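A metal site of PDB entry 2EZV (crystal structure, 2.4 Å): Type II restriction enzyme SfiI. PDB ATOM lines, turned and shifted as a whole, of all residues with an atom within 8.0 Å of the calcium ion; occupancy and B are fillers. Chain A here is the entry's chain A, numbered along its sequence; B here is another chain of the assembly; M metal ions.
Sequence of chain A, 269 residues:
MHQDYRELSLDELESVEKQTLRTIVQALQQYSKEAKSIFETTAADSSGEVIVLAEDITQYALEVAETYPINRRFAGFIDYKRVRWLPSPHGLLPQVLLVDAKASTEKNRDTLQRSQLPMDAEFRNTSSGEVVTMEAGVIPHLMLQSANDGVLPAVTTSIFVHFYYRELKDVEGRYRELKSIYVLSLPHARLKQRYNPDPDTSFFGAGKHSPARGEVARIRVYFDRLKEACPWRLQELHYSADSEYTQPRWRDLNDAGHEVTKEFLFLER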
ATOM      1  N   ILE A  51      25.341  20.041  15.167  1.00  0.00           N
ATOM      2  CA  ILE A  51      25.794  19.901  13.793  1.00  0.00           C
ATOM      3  C   ILE A  51      24.816  19.010  13.018  1.00  0.00           C
ATOM      4  O   ILE A  51      24.277  19.416  11.990  1.00  0.00           O
ATOM      5  CB  ILE A  51      27.174  19.240  13.730  1.00  0.00           C
ATOM      6  CG1 ILE A  51      28.214  20.097  14.471  1.00  0.00           C
ATOM      7  CG2 ILE A  51      27.573  19.027  12.276  1.00  0.00           C
ATOM      8  CD1 ILE A  51      29.572  19.456  14.574  1.00  0.00           C
ATOM      9  N   ALA A  54      21.151  20.331  12.803  1.00  0.00           N
ATOM     10  CA  ALA A  54      20.961  21.321  11.759  1.00  0.00           C
ATOM     11  C   ALA A  54      20.880  20.673  10.377  1.00  0.00           C
ATOM     12  O   ALA A  54      20.028  21.047   9.564  1.00  0.00           O
ATOM     13  CB  ALA A  54      22.095  22.342  11.801  1.00  0.00           C
ATOM     14  N   GLU A  55      21.745  19.704  10.111  1.00  0.00           N
ATOM     15  CA  GLU A  55      21.735  19.012   8.818  1.00  0.00           C
ATOM     16  C   GLU A  55      20.445  18.225   8.630  1.00  0.00           C
ATOM     17  O   GLU A  55      19.793  18.347   7.597  1.00  0.00           O
ATOM     18  CB  GLU A  55      22.941  18.069   8.710  1.00  0.00           C
ATOM     19  CG  GLU A  55      24.272  18.757   8.965  1.00  0.00           C
ATOM     20  CD  GLU A  55      25.462  17.818   8.819  1.00  0.00           C
ATOM     21  OE1 GLU A  55      25.358  16.639   9.238  1.00  0.00           O
ATOM     22  OE2 GLU A  55      26.506  18.248   8.293  1.00  0.00           O
ATOM     23  N   PHE A  77      30.784  17.348  -0.839  1.00  0.00           N
ATOM     24  CA  PHE A  77      30.731  18.059   0.431  1.00  0.00           C
ATOM     25  C   PHE A  77      29.671  19.142   0.513  1.00  0.00           C
ATOM     26  O   PHE A  77      29.984  20.323   0.679  1.00  0.00           O
ATOM     27  CB  PHE A  77      32.099  18.684   0.761  1.00  0.00           C
ATOM     28  CG  PHE A  77      33.090  17.714   1.330  1.00  0.00           C
ATOM     29  CD1 PHE A  77      33.991  17.048   0.510  1.00  0.00           C
ATOM     30  CD2 PHE A  77      33.113  17.448   2.712  1.00  0.00           C
ATOM     31  CE1 PHE A  77      34.916  16.133   1.039  1.00  0.00           C
ATOM     32  CE2 PHE A  77      34.028  16.540   3.257  1.00  0.00           C
ATOM     33  CZ  PHE A  77      34.930  15.873   2.413  1.00  0.00           C
ATOM     34  N   ILE A  78      28.411  18.745   0.384  1.00  0.00           N
ATOM     35  CA  ILE A  78      27.299  19.674   0.496  1.00  0.00           C
ATOM     36  C   ILE A  78      26.153  18.881   1.132  1.00  0.00           C
ATOM     37  O   ILE A  78      25.741  17.840   0.630  1.00  0.00           O
ATOM     38  CB  ILE A  78      26.873  20.253  -0.870  1.00  0.00           C
ATOM     39  CG1 ILE A  78      28.052  21.013  -1.484  1.00  0.00           C
ATOM     40  CG2 ILE A  78      25.685  21.207  -0.691  1.00  0.00           C
ATOM     41  CD1 ILE A  78      27.671  22.032  -2.537  1.00  0.00           C
ATOM     42  N   ASP A  79      25.674  19.375   2.268  1.00  0.00           N
ATOM     43  CA  ASP A  79      24.621  18.703   3.014  1.00  0.00           C
ATOM     44  C   ASP A  79      23.405  18.228   2.217  1.00  0.00           C
ATOM     45  O   ASP A  79      23.032  17.065   2.293  1.00  0.00           O
ATOM     46  CB  ASP A  79      24.146  19.589   4.167  1.00  0.00           C
ATOM     47  CG  ASP A  79      25.278  20.051   5.067  1.00  0.00           C
ATOM     48  OD1 ASP A  79      25.987  19.181   5.628  1.00  0.00           O
ATOM     49  OD2 ASP A  79      25.461  21.278   5.232  1.00  0.00           O
ATOM     50  N   TYR A  80      22.789  19.117   1.443  1.00  0.00           N
ATOM     51  CA  TYR A  80      21.591  18.792   0.684  1.00  0.00           C
ATOM     52  C   TYR A  80      21.728  19.131  -0.801  1.00  0.00           C
ATOM     53  O   TYR A  80      22.061  20.270  -1.145  1.00  0.00           O
ATOM     54  CB  TYR A  80      20.408  19.548   1.300  1.00  0.00           C
ATOM     55  CG  TYR A  80      19.054  19.239   0.697  1.00  0.00           C
ATOM     56  CD1 TYR A  80      18.268  18.186   1.168  1.00  0.00           C
ATOM     57  CD2 TYR A  80      18.543  20.021  -0.330  1.00  0.00           C
ATOM     58  CE1 TYR A  80      17.005  17.932   0.626  1.00  0.00           C
ATOM     59  CE2 TYR A  80      17.284  19.774  -0.883  1.00  0.00           C
ATOM     60  CZ  TYR A  80      16.524  18.727  -0.399  1.00  0.00           C
ATOM     61  OH  TYR A  80      15.286  18.500  -0.935  1.00  0.00           O
ATOM     62  N   VAL A  99      22.205  23.182  -0.893  1.00  0.00           N
ATOM     63  CA  VAL A  99      21.968  23.918   0.336  1.00  0.00           C
ATOM     64  C   VAL A  99      22.812  23.308   1.430  1.00  0.00           C
ATOM     65  O   VAL A  99      22.853  22.088   1.593  1.00  0.00           O
ATOM     66  CB  VAL A  99      20.464  23.913   0.744  1.00  0.00           C
ATOM     67  CG1 VAL A  99      19.571  23.847  -0.480  1.00  0.00           C
ATOM     68  CG2 VAL A  99      20.180  22.781   1.682  1.00  0.00           C
ATOM     69  N   ASP A 100      23.512  24.150   2.185  1.00  0.00           N
ATOM     70  CA  ASP A 100      24.347  23.676   3.267  1.00  0.00           C
ATOM     71  C   ASP A 100      23.821  24.196   4.589  1.00  0.00           C
ATOM     72  O   ASP A 100      23.350  25.327   4.676  1.00  0.00           O
ATOM     73  CB  ASP A 100      25.787  24.149   3.052  1.00  0.00           C
ATOM     74  CG  ASP A 100      26.788  23.230   3.707  1.00  0.00           C
ATOM     75  OD1 ASP A 100      27.318  23.594   4.789  1.00  0.00           O
ATOM     76  OD2 ASP A 100      27.029  22.143   3.140  1.00  0.00           O
ATOM     77  N   ALA A 101      23.897  23.354   5.613  1.00  0.00           N
ATOM     78  CA  ALA A 101      23.408  23.685   6.948  1.00  0.00           C
ATOM     79  C   ALA A 101      24.542  24.101   7.893  1.00  0.00           C
ATOM     80  O   ALA A 101      25.667  23.609   7.798  1.00  0.00           O
ATOM     81  CB  ALA A 101      22.665  22.495   7.527  1.00  0.00           C
ATOM     82  N   LYS A 102      24.219  25.009   8.808  1.00  0.00           N
ATOM     83  CA  LYS A 102      25.202  25.503   9.775  1.00  0.00           C
ATOM     84  C   LYS A 102      24.531  25.683  11.144  1.00  0.00           C
ATOM     85  O   LYS A 102      23.438  26.221  11.240  1.00  0.00           O
ATOM     86  CB  LYS A 102      25.759  26.868   9.344  1.00  0.00           C
ATOM     87  CG  LYS A 102      26.254  26.967   7.910  1.00  0.00           C
ATOM     88  CD  LYS A 102      27.645  26.355   7.709  1.00  0.00           C
ATOM     89  CE  LYS A 102      28.115  26.548   6.270  1.00  0.00           C
ATOM     90  NZ  LYS A 102      29.461  25.927   5.981  1.00  0.00           N
ATOM     91  N   ALA A 103      25.182  25.217  12.193  1.00  0.00           N
ATOM     92  CA  ALA A 103      24.653  25.429  13.539  1.00  0.00           C
ATOM     93  C   ALA A 103      25.614  26.493  14.069  1.00  0.00           C
ATOM     94  O   ALA A 103      26.813  26.421  13.798  1.00  0.00           O
ATOM     95  CB  ALA A 103      24.749  24.158  14.363  1.00  0.00           C
ATOM     96  N   THR A 111      30.392  30.694   7.883  1.00  0.00           N
ATOM     97  CA  THR A 111      31.674  30.201   7.399  1.00  0.00           C
ATOM     98  C   THR A 111      31.433  29.234   6.235  1.00  0.00           C
ATOM     99  O   THR A 111      30.465  28.467   6.245  1.00  0.00           O
ATOM    100  CB  THR A 111      32.462  29.448   8.503  1.00  0.00           C
ATOM    101  OG1 THR A 111      32.641  30.304   9.648  1.00  0.00           O
ATOM    102  CG2 THR A 111      33.833  29.041   7.978  1.00  0.00           C
ATOM    103  N   GLN A 113      33.424  26.470   3.294  1.00  0.00           N
ATOM    104  CA  GLN A 113      34.619  25.752   2.834  1.00  0.00           C
ATOM    105  C   GLN A 113      34.726  26.214   1.380  1.00  0.00           C
ATOM    106  O   GLN A 113      33.747  26.694   0.819  1.00  0.00           O
ATOM    107  CB  GLN A 113      34.403  24.224   2.835  1.00  0.00           C
ATOM    108  CG  GLN A 113      33.985  23.602   4.168  1.00  0.00           C
ATOM    109  CD  GLN A 113      35.040  23.750   5.260  1.00  0.00           C
ATOM    110  OE1 GLN A 113      36.197  23.351   5.098  1.00  0.00           O
ATOM    111  NE2 GLN A 113      34.630  24.334   6.392  1.00  0.00           N
ATOM    112  N   GLN A 116      32.059  25.113  -0.932  1.00  0.00           N
ATOM    113  CA  GLN A 116      30.693  25.615  -0.806  1.00  0.00           C
ATOM    114  C   GLN A 116      30.617  27.044  -1.355  1.00  0.00           C
ATOM    115  O   GLN A 116      29.568  27.683  -1.310  1.00  0.00           O
ATOM    116  CB  GLN A 116      30.255  25.580   0.662  1.00  0.00           C
ATOM    117  CG  GLN A 116      30.539  24.269   1.371  1.00  0.00           C
ATOM    118  CD  GLN A 116      30.377  24.342   2.897  1.00  0.00           C
ATOM    119  OE1 GLN A 116      30.545  25.402   3.498  1.00  0.00           O
ATOM    120  NE2 GLN A 116      30.071  23.209   3.519  1.00  0.00           N
ATOM    121  N   PHE A 160      22.063  28.660   2.001  1.00  0.00           N
ATOM    122  CA  PHE A 160      22.604  28.262   3.291  1.00  0.00           C
ATOM    123  C   PHE A 160      21.529  28.439   4.340  1.00  0.00           C
ATOM    124  O   PHE A 160      20.822  29.427   4.335  1.00  0.00           O
ATOM    125  CB  PHE A 160      23.846  29.103   3.653  1.00  0.00           C
ATOM    126  CG  PHE A 160      25.037  28.822   2.797  1.00  0.00           C
ATOM    127  CD1 PHE A 160      25.118  29.305   1.494  1.00  0.00           C
ATOM    128  CD2 PHE A 160      26.078  28.009   3.270  1.00  0.00           C
ATOM    129  CE1 PHE A 160      26.205  28.976   0.666  1.00  0.00           C
ATOM    130  CE2 PHE A 160      27.154  27.677   2.463  1.00  0.00           C
ATOM    131  CZ  PHE A 160      27.226  28.167   1.151  1.00  0.00           C
ATOM    132  N   VAL A 161      21.402  27.458   5.228  1.00  0.00           N
ATOM    133  CA  VAL A 161      20.409  27.501   6.284  1.00  0.00           C
ATOM    134  C   VAL A 161      21.222  27.535   7.570  1.00  0.00           C
ATOM    135  O   VAL A 161      21.978  26.615   7.867  1.00  0.00           O
ATOM    136  CB  VAL A 161      19.493  26.269   6.254  1.00  0.00           C
ATOM    137  CG1 VAL A 161      18.423  26.382   7.332  1.00  0.00           C
ATOM    138  CG2 VAL A 161      18.853  26.144   4.890  1.00  0.00           C
ATOM    139  P    DT B  12      37.916  18.901   5.354  1.00  0.00           P
ATOM    140  OP1  DT B  12      37.138  19.152   4.111  1.00  0.00           O
ATOM    141  OP2  DT B  12      38.918  19.897   5.800  1.00  0.00           O
ATOM    142  O5'  DT B  12      36.897  18.640   6.544  1.00  0.00           O
ATOM    143  C5'  DT B  12      36.248  17.375   6.648  1.00  0.00           C
ATOM    144  C4'  DT B  12      35.086  17.451   7.607  1.00  0.00           C
ATOM    145  O4'  DT B  12      35.581  17.488   8.965  1.00  0.00           O
ATOM    146  C3'  DT B  12      34.282  18.735   7.443  1.00  0.00           C
ATOM    147  O3'  DT B  12      32.912  18.485   7.800  1.00  0.00           O
ATOM    148  C2'  DT B  12      34.973  19.698   8.394  1.00  0.00           C
ATOM    149  C1'  DT B  12      35.355  18.770   9.550  1.00  0.00           C
ATOM    150  N1   DT B  12      36.544  19.135  10.350  1.00  0.00           N
ATOM    151  C2   DT B  12      36.451  19.035  11.727  1.00  0.00           C
ATOM    152  O2   DT B  12      35.441  18.657  12.316  1.00  0.00           O
ATOM    153  N3   DT B  12      37.588  19.388  12.410  1.00  0.00           N
ATOM    154  C4   DT B  12      38.775  19.831  11.870  1.00  0.00           C
ATOM    155  O4   DT B  12      39.717  20.119  12.606  1.00  0.00           O
ATOM    156  C5   DT B  12      38.805  19.916  10.421  1.00  0.00           C
ATOM    157  C7   DT B  12      40.054  20.389   9.744  1.00  0.00           C
ATOM    158  C6   DT B  12      37.699  19.567   9.743  1.00  0.00           C
ATOM    159  P    DT B  13      31.766  19.532   7.376  1.00  0.00           P
ATOM    160  OP1  DT B  13      30.650  18.749   6.783  1.00  0.00           O
ATOM    161  OP2  DT B  13      32.370  20.652   6.611  1.00  0.00           O
ATOM    162  O5'  DT B  13      31.269  20.098   8.773  1.00  0.00           O
ATOM    163  C5'  DT B  13      32.185  20.188   9.851  1.00  0.00           C
ATOM    164  C4'  DT B  13      31.499  20.684  11.093  1.00  0.00           C
ATOM    165  O4'  DT B  13      32.522  20.812  12.098  1.00  0.00           O
ATOM    166  C3'  DT B  13      30.874  22.066  10.953  1.00  0.00           C
ATOM    167  O3'  DT B  13      29.764  22.152  11.853  1.00  0.00           O
ATOM    168  C2'  DT B  13      32.030  22.984  11.303  1.00  0.00           C
ATOM    169  C1'  DT B  13      32.831  22.183  12.321  1.00  0.00           C
ATOM    170  N1   DT B  13      34.309  22.342  12.210  1.00  0.00           N
ATOM    171  C2   DT B  13      35.032  22.321  13.386  1.00  0.00           C
ATOM    172  O2   DT B  13      34.512  22.156  14.478  1.00  0.00           O
ATOM    173  N3   DT B  13      36.380  22.503  13.244  1.00  0.00           N
ATOM    174  C4   DT B  13      37.081  22.691  12.057  1.00  0.00           C
ATOM    175  O4   DT B  13      38.310  22.855  12.111  1.00  0.00           O
ATOM    176  C5   DT B  13      36.268  22.681  10.849  1.00  0.00           C
ATOM    177  C7   DT B  13      36.944  22.875   9.506  1.00  0.00           C
ATOM    178  C6   DT B  13      34.942  22.511  10.987  1.00  0.00           C
ATOM    179  P    DG B  14      28.777  23.413  11.807  1.00  0.00           P
ATOM    180  OP1  DG B  14      27.393  22.942  11.554  1.00  0.00           O
ATOM    181  OP2  DG B  14      29.349  24.480  10.955  1.00  0.00           O
ATOM    182  O5'  DG B  14      28.794  23.895  13.317  1.00  0.00           O
ATOM    183  C5'  DG B  14      29.321  25.163  13.648  1.00  0.00           C
ATOM    184  C4'  DG B  14      29.953  25.113  15.016  1.00  0.00           C
ATOM    185  O4'  DG B  14      31.339  24.682  14.900  1.00  0.00           O
ATOM    186  C3'  DG B  14      30.036  26.544  15.548  1.00  0.00           C
ATOM    187  O3'  DG B  14      30.123  26.491  16.958  1.00  0.00           O
ATOM    188  C2'  DG B  14      31.359  27.030  15.014  1.00  0.00           C
ATOM    189  C1'  DG B  14      32.187  25.781  15.179  1.00  0.00           C
ATOM    190  N9   DG B  14      33.373  25.736  14.336  1.00  0.00           N
ATOM    191  C8   DG B  14      33.465  25.784  12.967  1.00  0.00           C
ATOM    192  N7   DG B  14      34.691  25.844  12.546  1.00  0.00           N
ATOM    193  C5   DG B  14      35.454  25.830  13.707  1.00  0.00           C
ATOM    194  C6   DG B  14      36.856  25.886  13.891  1.00  0.00           C
ATOM    195  O6   DG B  14      37.743  25.988  13.023  1.00  0.00           O
ATOM    196  N1   DG B  14      37.196  25.832  15.238  1.00  0.00           N
ATOM    197  C2   DG B  14      36.296  25.733  16.286  1.00  0.00           C
ATOM    198  N2   DG B  14      36.793  25.694  17.525  1.00  0.00           N
ATOM    199  N3   DG B  14      34.992  25.686  16.110  1.00  0.00           N
ATOM    200  C4   DG B  14      34.641  25.729  14.812  1.00  0.00           C
HETATM  201 CA    CA M   1      27.176  22.127   6.697  1.00  0.00          CA
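The side-chain carboxylate (OD1) of Asp 100 lies close to the side-chain amino group (NZ) of Lys 102 (3.4 Å).
The side-chain carboxylate (OD2) of Asp 100 lies within hydrogen-bond range of the side-chain amide nitrogen (NE2) of Gln 116.
The backbone carbonyl oxygen of Asp 100 sits at hydrogen-bond distance from the backbone NH of Val 161.
Three residues have an atom within 4 Å of the calcium ion: Asp 79, Asp 100 and Ala 101.
The nearest printed residue that does not touch the calcium ion is Glu 55 (4.2 Å).
The calcium ion is bound by O of Ala 101 (2.4 Å).
OD2 of Asp 79 is bound to the calcium ion (2.4 Å).
The calcium ion is bound by the side-chain carboxylate (OD1) of Asp 100 (2.4 Å).
The calcium ion has three donor atoms within binding distance.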
